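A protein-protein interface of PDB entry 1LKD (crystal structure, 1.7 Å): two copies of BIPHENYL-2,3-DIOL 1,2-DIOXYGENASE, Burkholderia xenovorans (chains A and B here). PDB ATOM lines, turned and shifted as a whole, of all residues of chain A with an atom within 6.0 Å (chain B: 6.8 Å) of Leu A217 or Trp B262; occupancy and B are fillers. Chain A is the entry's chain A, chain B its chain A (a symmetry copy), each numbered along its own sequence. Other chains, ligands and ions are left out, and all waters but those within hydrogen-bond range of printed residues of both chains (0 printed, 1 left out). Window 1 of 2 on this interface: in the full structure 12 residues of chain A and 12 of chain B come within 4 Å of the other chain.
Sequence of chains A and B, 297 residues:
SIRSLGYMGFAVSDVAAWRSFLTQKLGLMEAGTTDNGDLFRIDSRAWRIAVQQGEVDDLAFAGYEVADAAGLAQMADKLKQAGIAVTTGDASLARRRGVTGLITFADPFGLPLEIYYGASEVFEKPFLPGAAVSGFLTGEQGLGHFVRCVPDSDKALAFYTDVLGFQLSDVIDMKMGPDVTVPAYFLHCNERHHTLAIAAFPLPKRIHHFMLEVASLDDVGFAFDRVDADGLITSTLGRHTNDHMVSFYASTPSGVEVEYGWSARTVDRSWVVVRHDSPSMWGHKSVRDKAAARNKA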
ATOM      1  N   ALA A 215       3.882   5.524   0.945  1.00  0.00           N
ATOM      2  CA  ALA A 215       3.307   6.569   0.102  1.00  0.00           C
ATOM      3  C   ALA A 215       4.208   7.627  -0.528  1.00  0.00           C
ATOM      4  O   ALA A 215       3.821   8.243  -1.518  1.00  0.00           O
ATOM      5  CB  ALA A 215       2.170   7.257   0.866  1.00  0.00           C
ATOM      6  N   SER A 216       5.397   7.852   0.018  1.00  0.00           N
ATOM      7  CA  SER A 216       6.272   8.864  -0.561  1.00  0.00           C
ATOM      8  C   SER A 216       7.726   8.433  -0.591  1.00  0.00           C
ATOM      9  O   SER A 216       8.123   7.501   0.112  1.00  0.00           O
ATOM     10  CB  SER A 216       6.169  10.166   0.229  1.00  0.00           C
ATOM     11  OG  SER A 216       6.828  10.037   1.474  1.00  0.00           O
ATOM     12  N   LEU A 217       8.516   9.120  -1.411  1.00  0.00           N
ATOM     13  CA  LEU A 217       9.938   8.831  -1.513  1.00  0.00           C
ATOM     14  C   LEU A 217      10.609   9.133  -0.174  1.00  0.00           C
ATOM     15  O   LEU A 217      11.506   8.404   0.253  1.00  0.00           O
ATOM     16  CB  LEU A 217      10.578   9.680  -2.614  1.00  0.00           C
ATOM     17  CG  LEU A 217      12.108   9.643  -2.686  1.00  0.00           C
ATOM     18  CD1 LEU A 217      12.593   8.220  -2.942  1.00  0.00           C
ATOM     19  CD2 LEU A 217      12.573  10.562  -3.799  1.00  0.00           C
ATOM     20  N   ASP A 218      10.180  10.205   0.488  1.00  0.00           N
ATOM     21  CA  ASP A 218      10.766  10.552   1.780  1.00  0.00           C
ATOM     22  C   ASP A 218      10.542   9.439   2.804  1.00  0.00           C
ATOM     23  O   ASP A 218      11.393   9.200   3.652  1.00  0.00           O
ATOM     24  CB  ASP A 218      10.191  11.866   2.315  1.00  0.00           C
ATOM     25  CG  ASP A 218      10.721  13.076   1.574  1.00  0.00           C
ATOM     26  OD1 ASP A 218      11.851  13.004   1.045  1.00  0.00           O
ATOM     27  OD2 ASP A 218      10.015  14.107   1.536  1.00  0.00           O
ATOM     28  N   ASP A 219       9.397   8.764   2.738  1.00  0.00           N
ATOM     29  CA  ASP A 219       9.159   7.671   3.680  1.00  0.00           C
ATOM     30  C   ASP A 219      10.292   6.658   3.540  1.00  0.00           C
ATOM     31  O   ASP A 219      10.820   6.157   4.533  1.00  0.00           O
ATOM     32  CB  ASP A 219       7.826   6.970   3.402  1.00  0.00           C
ATOM     33  CG  ASP A 219       6.630   7.840   3.717  1.00  0.00           C
ATOM     34  OD1 ASP A 219       6.749   8.723   4.596  1.00  0.00           O
ATOM     35  OD2 ASP A 219       5.563   7.624   3.101  1.00  0.00           O
ATOM     36  N   VAL A 220      10.661   6.358   2.299  1.00  0.00           N
ATOM     37  CA  VAL A 220      11.739   5.411   2.041  1.00  0.00           C
ATOM     38  C   VAL A 220      13.088   5.984   2.481  1.00  0.00           C
ATOM     39  O   VAL A 220      13.863   5.307   3.156  1.00  0.00           O
ATOM     40  CB  VAL A 220      11.815   5.050   0.540  1.00  0.00           C
ATOM     41  CG1 VAL A 220      12.925   4.036   0.308  1.00  0.00           C
ATOM     42  CG2 VAL A 220      10.479   4.485   0.073  1.00  0.00           C
ATOM     43  N   GLY A 221      13.356   7.230   2.098  1.00  0.00           N
ATOM     44  CA  GLY A 221      14.614   7.876   2.453  1.00  0.00           C
ATOM     45  C   GLY A 221      14.895   7.949   3.945  1.00  0.00           C
ATOM     46  O   GLY A 221      16.011   7.660   4.395  1.00  0.00           O
ATOM     47  N   PHE A 222      13.889   8.341   4.721  1.00  0.00           N
ATOM     48  CA  PHE A 222      14.047   8.434   6.168  1.00  0.00           C
ATOM     49  C   PHE A 222      14.243   7.048   6.776  1.00  0.00           C
ATOM     50  O   PHE A 222      15.085   6.865   7.650  1.00  0.00           O
ATOM     51  CB  PHE A 222      12.825   9.105   6.805  1.00  0.00           C
ATOM     52  CG  PHE A 222      12.799  10.603   6.647  1.00  0.00           C
ATOM     53  CD1 PHE A 222      13.828  11.389   7.161  1.00  0.00           C
ATOM     54  CD2 PHE A 222      11.735  11.233   6.005  1.00  0.00           C
ATOM     55  CE1 PHE A 222      13.796  12.781   7.043  1.00  0.00           C
ATOM     56  CE2 PHE A 222      11.693  12.625   5.880  1.00  0.00           C
ATOM     57  CZ  PHE A 222      12.727  13.400   6.403  1.00  0.00           C
ATOM     58  N   LEU A 237      19.614   2.212  -2.257  1.00  0.00           N
ATOM     59  CA  LEU A 237      18.379   2.574  -2.945  1.00  0.00           C
ATOM     60  C   LEU A 237      18.511   2.266  -4.438  1.00  0.00           C
ATOM     61  O   LEU A 237      19.563   2.494  -5.035  1.00  0.00           O
ATOM     62  CB  LEU A 237      18.090   4.063  -2.768  1.00  0.00           C
ATOM     63  CG  LEU A 237      17.718   4.573  -1.376  1.00  0.00           C
ATOM     64  CD1 LEU A 237      17.698   6.094  -1.394  1.00  0.00           C
ATOM     65  CD2 LEU A 237      16.352   4.025  -0.962  1.00  0.00           C
ATOM     66  N   VAL A 246      10.906   1.847  -6.292  1.00  0.00           N
ATOM     67  CA  VAL A 246      12.152   2.426  -5.779  1.00  0.00           C
ATOM     68  C   VAL A 246      12.204   1.901  -4.348  1.00  0.00           C
ATOM     69  O   VAL A 246      11.289   2.152  -3.563  1.00  0.00           O
ATOM     70  CB  VAL A 246      12.106   3.969  -5.753  1.00  0.00           C
ATOM     71  CG1 VAL A 246      13.340   4.515  -5.041  1.00  0.00           C
ATOM     72  CG2 VAL A 246      12.056   4.511  -7.177  1.00  0.00           C
ATOM     73  N   TRP A 262       8.627   2.411  -2.787  1.00  0.00           N
ATOM     74  CA  TRP A 262       7.675   3.427  -3.215  1.00  0.00           C
ATOM     75  C   TRP A 262       7.577   3.578  -4.740  1.00  0.00           C
ATOM     76  O   TRP A 262       8.548   3.354  -5.458  1.00  0.00           O
ATOM     77  CB  TRP A 262       8.116   4.765  -2.603  1.00  0.00           C
ATOM     78  CG  TRP A 262       7.549   5.998  -3.259  1.00  0.00           C
ATOM     79  CD1 TRP A 262       6.326   6.561  -3.031  1.00  0.00           C
ATOM     80  CD2 TRP A 262       8.191   6.818  -4.244  1.00  0.00           C
ATOM     81  NE1 TRP A 262       6.167   7.678  -3.809  1.00  0.00           N
ATOM     82  CE2 TRP A 262       7.294   7.861  -4.566  1.00  0.00           C
ATOM     83  CE3 TRP A 262       9.435   6.772  -4.887  1.00  0.00           C
ATOM     84  CZ2 TRP A 262       7.601   8.854  -5.507  1.00  0.00           C
ATOM     85  CZ3 TRP A 262       9.741   7.762  -5.826  1.00  0.00           C
ATOM     86  CH2 TRP A 262       8.825   8.786  -6.124  1.00  0.00           C
ATOM     87  N   MET B 211      25.938  22.767  -9.589  1.00  0.00           N
ATOM     88  CA  MET B 211      24.823  21.829  -9.613  1.00  0.00           C
ATOM     89  C   MET B 211      23.990  21.926 -10.878  1.00  0.00           C
ATOM     90  O   MET B 211      23.743  23.019 -11.385  1.00  0.00           O
ATOM     91  CB  MET B 211      23.929  22.090  -8.388  1.00  0.00           C
ATOM     92  CG  MET B 211      22.757  21.122  -8.173  1.00  0.00           C
ATOM     93  SD  MET B 211      21.295  21.399  -9.212  1.00  0.00           S
ATOM     94  CE  MET B 211      20.802  22.996  -8.729  1.00  0.00           C
ATOM     95  N   LEU B 212      23.574  20.769 -11.385  1.00  0.00           N
ATOM     96  CA  LEU B 212      22.723  20.700 -12.564  1.00  0.00           C
ATOM     97  C   LEU B 212      21.480  19.922 -12.141  1.00  0.00           C
ATOM     98  O   LEU B 212      21.585  18.900 -11.456  1.00  0.00           O
ATOM     99  CB  LEU B 212      23.433  19.978 -13.715  1.00  0.00           C
ATOM    100  CG  LEU B 212      24.689  20.657 -14.272  1.00  0.00           C
ATOM    101  CD1 LEU B 212      25.216  19.846 -15.443  1.00  0.00           C
ATOM    102  CD2 LEU B 212      24.368  22.085 -14.718  1.00  0.00           C
ATOM    103  N   GLU B 213      20.308  20.407 -12.535  1.00  0.00           N
ATOM    104  CA  GLU B 213      19.059  19.749 -12.170  1.00  0.00           C
ATOM    105  C   GLU B 213      18.423  19.057 -13.372  1.00  0.00           C
ATOM    106  O   GLU B 213      18.382  19.617 -14.469  1.00  0.00           O
ATOM    107  CB  GLU B 213      18.080  20.768 -11.568  1.00  0.00           C
ATOM    108  CG  GLU B 213      16.746  20.169 -11.150  1.00  0.00           C
ATOM    109  CD  GLU B 213      15.872  21.146 -10.375  1.00  0.00           C
ATOM    110  OE1 GLU B 213      16.252  22.331 -10.260  1.00  0.00           O
ATOM    111  OE2 GLU B 213      14.801  20.724  -9.880  1.00  0.00           O
ATOM    112  N   VAL B 214      17.942  17.836 -13.156  1.00  0.00           N
ATOM    113  CA  VAL B 214      17.313  17.055 -14.214  1.00  0.00           C
ATOM    114  C   VAL B 214      15.816  16.895 -13.981  1.00  0.00           C
ATOM    115  O   VAL B 214      15.311  17.179 -12.894  1.00  0.00           O
ATOM    116  CB  VAL B 214      17.987  15.669 -14.366  1.00  0.00           C
ATOM    117  CG1 VAL B 214      19.354  15.835 -15.017  1.00  0.00           C
ATOM    118  CG2 VAL B 214      18.142  15.003 -13.003  1.00  0.00           C
ATOM    119  N   ALA B 215      15.115  16.422 -15.007  1.00  0.00           N
ATOM    120  CA  ALA B 215      13.661  16.291 -14.968  1.00  0.00           C
ATOM    121  C   ALA B 215      13.017  15.117 -14.237  1.00  0.00           C
ATOM    122  O   ALA B 215      11.849  15.202 -13.863  1.00  0.00           O
ATOM    123  CB  ALA B 215      13.116  16.361 -16.400  1.00  0.00           C
ATOM    124  N   SER B 216      13.745  14.029 -14.023  1.00  0.00           N
ATOM    125  CA  SER B 216      13.149  12.891 -13.333  1.00  0.00           C
ATOM    126  C   SER B 216      14.101  12.238 -12.350  1.00  0.00           C
ATOM    127  O   SER B 216      15.315  12.444 -12.413  1.00  0.00           O
ATOM    128  CB  SER B 216      12.698  11.838 -14.343  1.00  0.00           C
ATOM    129  OG  SER B 216      13.819  11.165 -14.881  1.00  0.00           O
ATOM    130  N   LEU B 217      13.540  11.448 -11.439  1.00  0.00           N
ATOM    131  CA  LEU B 217      14.340  10.735 -10.456  1.00  0.00           C
ATOM    132  C   LEU B 217      15.237   9.728 -11.173  1.00  0.00           C
ATOM    133  O   LEU B 217      16.391   9.532 -10.788  1.00  0.00           O
ATOM    134  CB  LEU B 217      13.438  10.005  -9.459  1.00  0.00           C
ATOM    135  CG  LEU B 217      14.140   9.036  -8.501  1.00  0.00           C
ATOM    136  CD1 LEU B 217      15.161   9.780  -7.648  1.00  0.00           C
ATOM    137  CD2 LEU B 217      13.101   8.376  -7.617  1.00  0.00           C
ATOM    138  N   ASP B 218      14.711   9.086 -12.215  1.00  0.00           N
ATOM    139  CA  ASP B 218      15.510   8.115 -12.958  1.00  0.00           C
ATOM    140  C   ASP B 218      16.738   8.775 -13.583  1.00  0.00           C
ATOM    141  O   ASP B 218      17.791   8.156 -13.676  1.00  0.00           O
ATOM    142  CB  ASP B 218      14.680   7.433 -14.049  1.00  0.00           C
ATOM    143  CG  ASP B 218      13.696   6.428 -13.488  1.00  0.00           C
ATOM    144  OD1 ASP B 218      13.968   5.868 -12.403  1.00  0.00           O
ATOM    145  OD2 ASP B 218      12.659   6.182 -14.140  1.00  0.00           O
ATOM    146  N   ASP B 219      16.609  10.024 -14.022  1.00  0.00           N
ATOM    147  CA  ASP B 219      17.769  10.702 -14.598  1.00  0.00           C
ATOM    148  C   ASP B 219      18.892  10.698 -13.564  1.00  0.00           C
ATOM    149  O   ASP B 219      20.051  10.439 -13.889  1.00  0.00           O
ATOM    150  CB  ASP B 219      17.445  12.149 -14.977  1.00  0.00           C
ATOM    151  CG  ASP B 219      16.489  12.249 -16.146  1.00  0.00           C
ATOM    152  OD1 ASP B 219      16.472  11.319 -16.983  1.00  0.00           O
ATOM    153  OD2 ASP B 219      15.771  13.269 -16.237  1.00  0.00           O
ATOM    154  N   VAL B 220      18.541  10.990 -12.316  1.00  0.00           N
ATOM    155  CA  VAL B 220      19.525  11.008 -11.241  1.00  0.00           C
ATOM    156  C   VAL B 220      20.037   9.597 -10.943  1.00  0.00           C
ATOM    157  O   VAL B 220      21.243   9.381 -10.833  1.00  0.00           O
ATOM    158  CB  VAL B 220      18.925  11.605  -9.948  1.00  0.00           C
ATOM    159  CG1 VAL B 220      19.984  11.642  -8.855  1.00  0.00           C
ATOM    160  CG2 VAL B 220      18.399  13.009 -10.219  1.00  0.00           C
ATOM    161  N   ARG B 239      18.303  13.981   0.232  1.00  0.00           N
ATOM    162  CA  ARG B 239      17.465  15.140  -0.050  1.00  0.00           C
ATOM    163  C   ARG B 239      17.865  16.248   0.906  1.00  0.00           C
ATOM    164  O   ARG B 239      18.016  16.018   2.107  1.00  0.00           O
ATOM    165  CB  ARG B 239      15.968  14.841   0.133  1.00  0.00           C
ATOM    166  CG  ARG B 239      15.099  15.986  -0.413  1.00  0.00           C
ATOM    167  CD  ARG B 239      13.653  15.953   0.074  1.00  0.00           C
ATOM    168  NE  ARG B 239      12.825  14.895  -0.502  1.00  0.00           N
ATOM    169  CZ  ARG B 239      12.184  14.966  -1.669  1.00  0.00           C
ATOM    170  NH1 ARG B 239      12.269  16.049  -2.430  1.00  0.00           N
ATOM    171  NH2 ARG B 239      11.415  13.958  -2.056  1.00  0.00           N
ATOM    172  N   HIS B 244      15.089  20.990  -0.655  1.00  0.00           N
ATOM    173  CA  HIS B 244      14.426  19.700  -0.833  1.00  0.00           C
ATOM    174  C   HIS B 244      14.766  18.983  -2.131  1.00  0.00           C
ATOM    175  O   HIS B 244      13.973  18.190  -2.641  1.00  0.00           O
ATOM    176  CB  HIS B 244      12.908  19.882  -0.717  1.00  0.00           C
ATOM    177  CG  HIS B 244      12.481  20.450   0.599  1.00  0.00           C
ATOM    178  ND1 HIS B 244      11.176  20.807   0.873  1.00  0.00           N
ATOM    179  CD2 HIS B 244      13.187  20.708   1.726  1.00  0.00           C
ATOM    180  CE1 HIS B 244      11.098  21.257   2.113  1.00  0.00           C
ATOM    181  NE2 HIS B 244      12.303  21.207   2.654  1.00  0.00           N
ATOM    182  N   MET B 245      15.953  19.261  -2.652  1.00  0.00           N
ATOM    183  CA  MET B 245      16.421  18.623  -3.876  1.00  0.00           C
ATOM    184  C   MET B 245      16.948  17.227  -3.536  1.00  0.00           C
ATOM    185  O   MET B 245      17.610  17.043  -2.507  1.00  0.00           O
ATOM    186  CB  MET B 245      17.564  19.444  -4.486  1.00  0.00           C
ATOM    187  CG  MET B 245      18.103  18.897  -5.801  1.00  0.00           C
ATOM    188  SD  MET B 245      17.212  19.560  -7.227  1.00  0.00           S
ATOM    189  CE  MET B 245      18.092  21.110  -7.467  1.00  0.00           C
ATOM    190  N   VAL B 246      16.637  16.249  -4.382  1.00  0.00           N
ATOM    191  CA  VAL B 246      17.139  14.882  -4.203  1.00  0.00           C
ATOM    192  C   VAL B 246      18.346  14.840  -5.135  1.00  0.00           C
ATOM    193  O   VAL B 246      18.206  15.064  -6.338  1.00  0.00           O
ATOM    194  CB  VAL B 246      16.110  13.823  -4.655  1.00  0.00           C
ATOM    195  CG1 VAL B 246      16.744  12.436  -4.627  1.00  0.00           C
ATOM    196  CG2 VAL B 246      14.898  13.850  -3.731  1.00  0.00           C
ATOM    197  N   SER B 247      19.524  14.547  -4.594  1.00  0.00           N
ATOM    198  CA  SER B 247      20.728  14.561  -5.411  1.00  0.00           C
ATOM    199  C   SER B 247      21.851  13.702  -4.858  1.00  0.00           C
ATOM    200  O   SER B 247      21.735  13.108  -3.792  1.00  0.00           O
ATOM    201  CB  SER B 247      21.254  15.991  -5.475  1.00  0.00           C
ATOM    202  OG  SER B 247      21.664  16.401  -4.167  1.00  0.00           O
ATOM    203  N   TYR B 260      24.139  16.596  -8.789  1.00  0.00           N
ATOM    204  CA  TYR B 260      23.186  16.237  -9.838  1.00  0.00           C
ATOM    205  C   TYR B 260      21.873  15.932  -9.121  1.00  0.00           C
ATOM    206  O   TYR B 260      21.774  14.935  -8.396  1.00  0.00           O
ATOM    207  CB  TYR B 260      23.729  14.996 -10.542  1.00  0.00           C
ATOM    208  CG  TYR B 260      23.251  14.750 -11.949  1.00  0.00           C
ATOM    209  CD1 TYR B 260      23.840  15.402 -13.036  1.00  0.00           C
ATOM    210  CD2 TYR B 260      22.268  13.799 -12.202  1.00  0.00           C
ATOM    211  CE1 TYR B 260      23.466  15.093 -14.348  1.00  0.00           C
ATOM    212  CE2 TYR B 260      21.885  13.488 -13.501  1.00  0.00           C
ATOM    213  CZ  TYR B 260      22.490  14.131 -14.565  1.00  0.00           C
ATOM    214  OH  TYR B 260      22.132  13.779 -15.841  1.00  0.00           O
ATOM    215  N   GLY B 261      20.863  16.777  -9.324  1.00  0.00           N
ATOM    216  CA  GLY B 261      19.617  16.581  -8.607  1.00  0.00           C
ATOM    217  C   GLY B 261      18.289  16.735  -9.312  1.00  0.00           C
ATOM    218  O   GLY B 261      18.214  17.143 -10.473  1.00  0.00           O
ATOM    219  N   TRP B 262      17.235  16.442  -8.554  1.00  0.00           N
ATOM    220  CA  TRP B 262      15.864  16.472  -9.047  1.00  0.00           C
ATOM    221  C   TRP B 262      14.829  16.832  -7.971  1.00  0.00           C
ATOM    222  O   TRP B 262      15.016  16.535  -6.794  1.00  0.00           O
ATOM    223  CB  TRP B 262      15.542  15.081  -9.612  1.00  0.00           C
ATOM    224  CG  TRP B 262      14.076  14.764  -9.762  1.00  0.00           C
ATOM    225  CD1 TRP B 262      13.261  15.119 -10.798  1.00  0.00           C
ATOM    226  CD2 TRP B 262      13.260  14.022  -8.845  1.00  0.00           C
ATOM    227  NE1 TRP B 262      11.991  14.645 -10.585  1.00  0.00           N
ATOM    228  CE2 TRP B 262      11.960  13.969  -9.394  1.00  0.00           C
ATOM    229  CE3 TRP B 262      13.501  13.399  -7.613  1.00  0.00           C
ATOM    230  CZ2 TRP B 262      10.898  13.316  -8.753  1.00  0.00           C
ATOM    231  CZ3 TRP B 262      12.443  12.748  -6.973  1.00  0.00           C
ATOM    232  CH2 TRP B 262      11.159  12.715  -7.547  1.00  0.00           C
ATOM    233  N   SER B 263      13.751  17.489  -8.399  1.00  0.00           N
ATOM    234  CA  SER B 263      12.618  17.830  -7.538  1.00  0.00           C
ATOM    235  C   SER B 263      12.760  18.894  -6.447  1.00  0.00           C
ATOM    236  O   SER B 263      12.062  18.834  -5.432  1.00  0.00           O
ATOM    237  CB  SER B 263      12.080  16.537  -6.911  1.00  0.00           C
ATOM    238  OG  SER B 263      10.800  16.725  -6.332  1.00  0.00           O
ATOM    239  N   ALA B 264      13.634  19.875  -6.639  1.00  0.00           N
ATOM    240  CA  ALA B 264      13.780  20.921  -5.629  1.00  0.00           C
ATOM    241  C   ALA B 264      12.546  21.822  -5.590  1.00  0.00           C
ATOM    242  O   ALA B 264      11.856  21.997  -6.600  1.00  0.00           O
ATOM    243  CB  ALA B 264      15.013  21.762  -5.920  1.00  0.00           C
ATOM    244  N   TRP B 282      17.737  13.337   4.643  1.00  0.00           N
ATOM    245  CA  TRP B 282      18.150  11.944   4.643  1.00  0.00           C
ATOM    246  C   TRP B 282      19.194  11.745   3.558  1.00  0.00           C
ATOM    247  O   TRP B 282      19.316  12.563   2.641  1.00  0.00           O
ATOM    248  CB  TRP B 282      16.958  10.989   4.421  1.00  0.00           C
ATOM    249  CG  TRP B 282      16.058  11.296   3.242  1.00  0.00           C
ATOM    250  CD1 TRP B 282      14.874  11.980   3.271  1.00  0.00           C
ATOM    251  CD2 TRP B 282      16.251  10.892   1.876  1.00  0.00           C
ATOM    252  NE1 TRP B 282      14.317  12.024   2.014  1.00  0.00           N
ATOM    253  CE2 TRP B 282      15.141  11.368   1.140  1.00  0.00           C
ATOM    254  CE3 TRP B 282      17.253  10.176   1.206  1.00  0.00           C
ATOM    255  CZ2 TRP B 282      15.002  11.150  -0.237  1.00  0.00           C
ATOM    256  CZ3 TRP B 282      17.116   9.957  -0.172  1.00  0.00           C
ATOM    257  CH2 TRP B 282      15.996  10.446  -0.874  1.00  0.00           C
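The side-chain carboxylate (OD1) of Asp A218 is in salt-bridge range of the guanidinium group (NE) of Arg B239, 2.6 Å away. OD1 of Asp A218 lies within hydrogen-bond range of NE1 of Trp B282 (2.8 Å).
Ala A215 touches none of the printed residues of chain B. Of the printed residues of chain B, Leu A217 touches Arg B239 and Trp B262. Of the printed residues of chain B, Gly A221 touches Trp B282. Printed residues of chain B within 4 Å of Phe A222: Trp B282 (3.95 Å). Of the printed residues of chain A, Trp B262 touches Leu A217 (3.9 Å). Of the printed residues of chain A, Trp B282 touches Asp A218, Gly A221 and Phe A222. The nearest residue of chain A that does not touch Trp B262 is Trp A262 (4.8 Å).
O of Ala A215 sits at hydrogen-bond distance from NE1 of Trp A262 (3.3 Å). The backbone NH of Trp A262 sits at hydrogen-bond distance from the backbone carbonyl oxygen of Val A246. O of His B244 lies within hydrogen-bond range of NH1 of Arg B239 (2.7 Å). N of Arg B239 lies within hydrogen-bond range of O of Trp B282. The side-chain sulfur (SD) of Met B245 is in hydrogen-bond range of the backbone NH (N) of Trp B262 (3.4 Å). The backbone carbonyl oxygen (O) of Val B246 sits at hydrogen-bond distance from the backbone NH (N) of Trp B262 (2.8 Å).
Leu A217 touches Trp B262, and with the chains exchanged Trp A262 touches Leu B217. Positions printed for both chains: 215, 216, 217, 218, 219, 220, 246 and 262. Of the 7 pairs that touch across the chains among the printed residues, 2 have their exchanged pair printed and touching as well.
Printed residues of chain A that touch a printed residue of chain B: Leu A217, Asp A218, Gly A221, Phe A222 and Trp A262. Hydrophobic or aromatic side chains of chain A that line the printed part of chain B: Leu A217 and Trp A262. Among the printed residues, 7 pairs touch across the chains. Among the printed residues, Asp or Glu carboxylates within 4 Å of a Lys or Arg side-chain nitrogen of the other chain: Asp A218 with Arg B239 (2.6 Å).
NH2 of Arg B239 touches CD2 of Leu A217 (3.99 Å). CD2 of Leu A217 touches CZ3 of Trp B262, at 3.9 Å. O of Gly A221 touches CB of Trp B282, 3.5 Å away. CG of Trp B282 touches N of Phe A222, 3.95 Å away. CD2 of Leu B217 touches CZ3 of Trp A262, 3.9 Å away.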
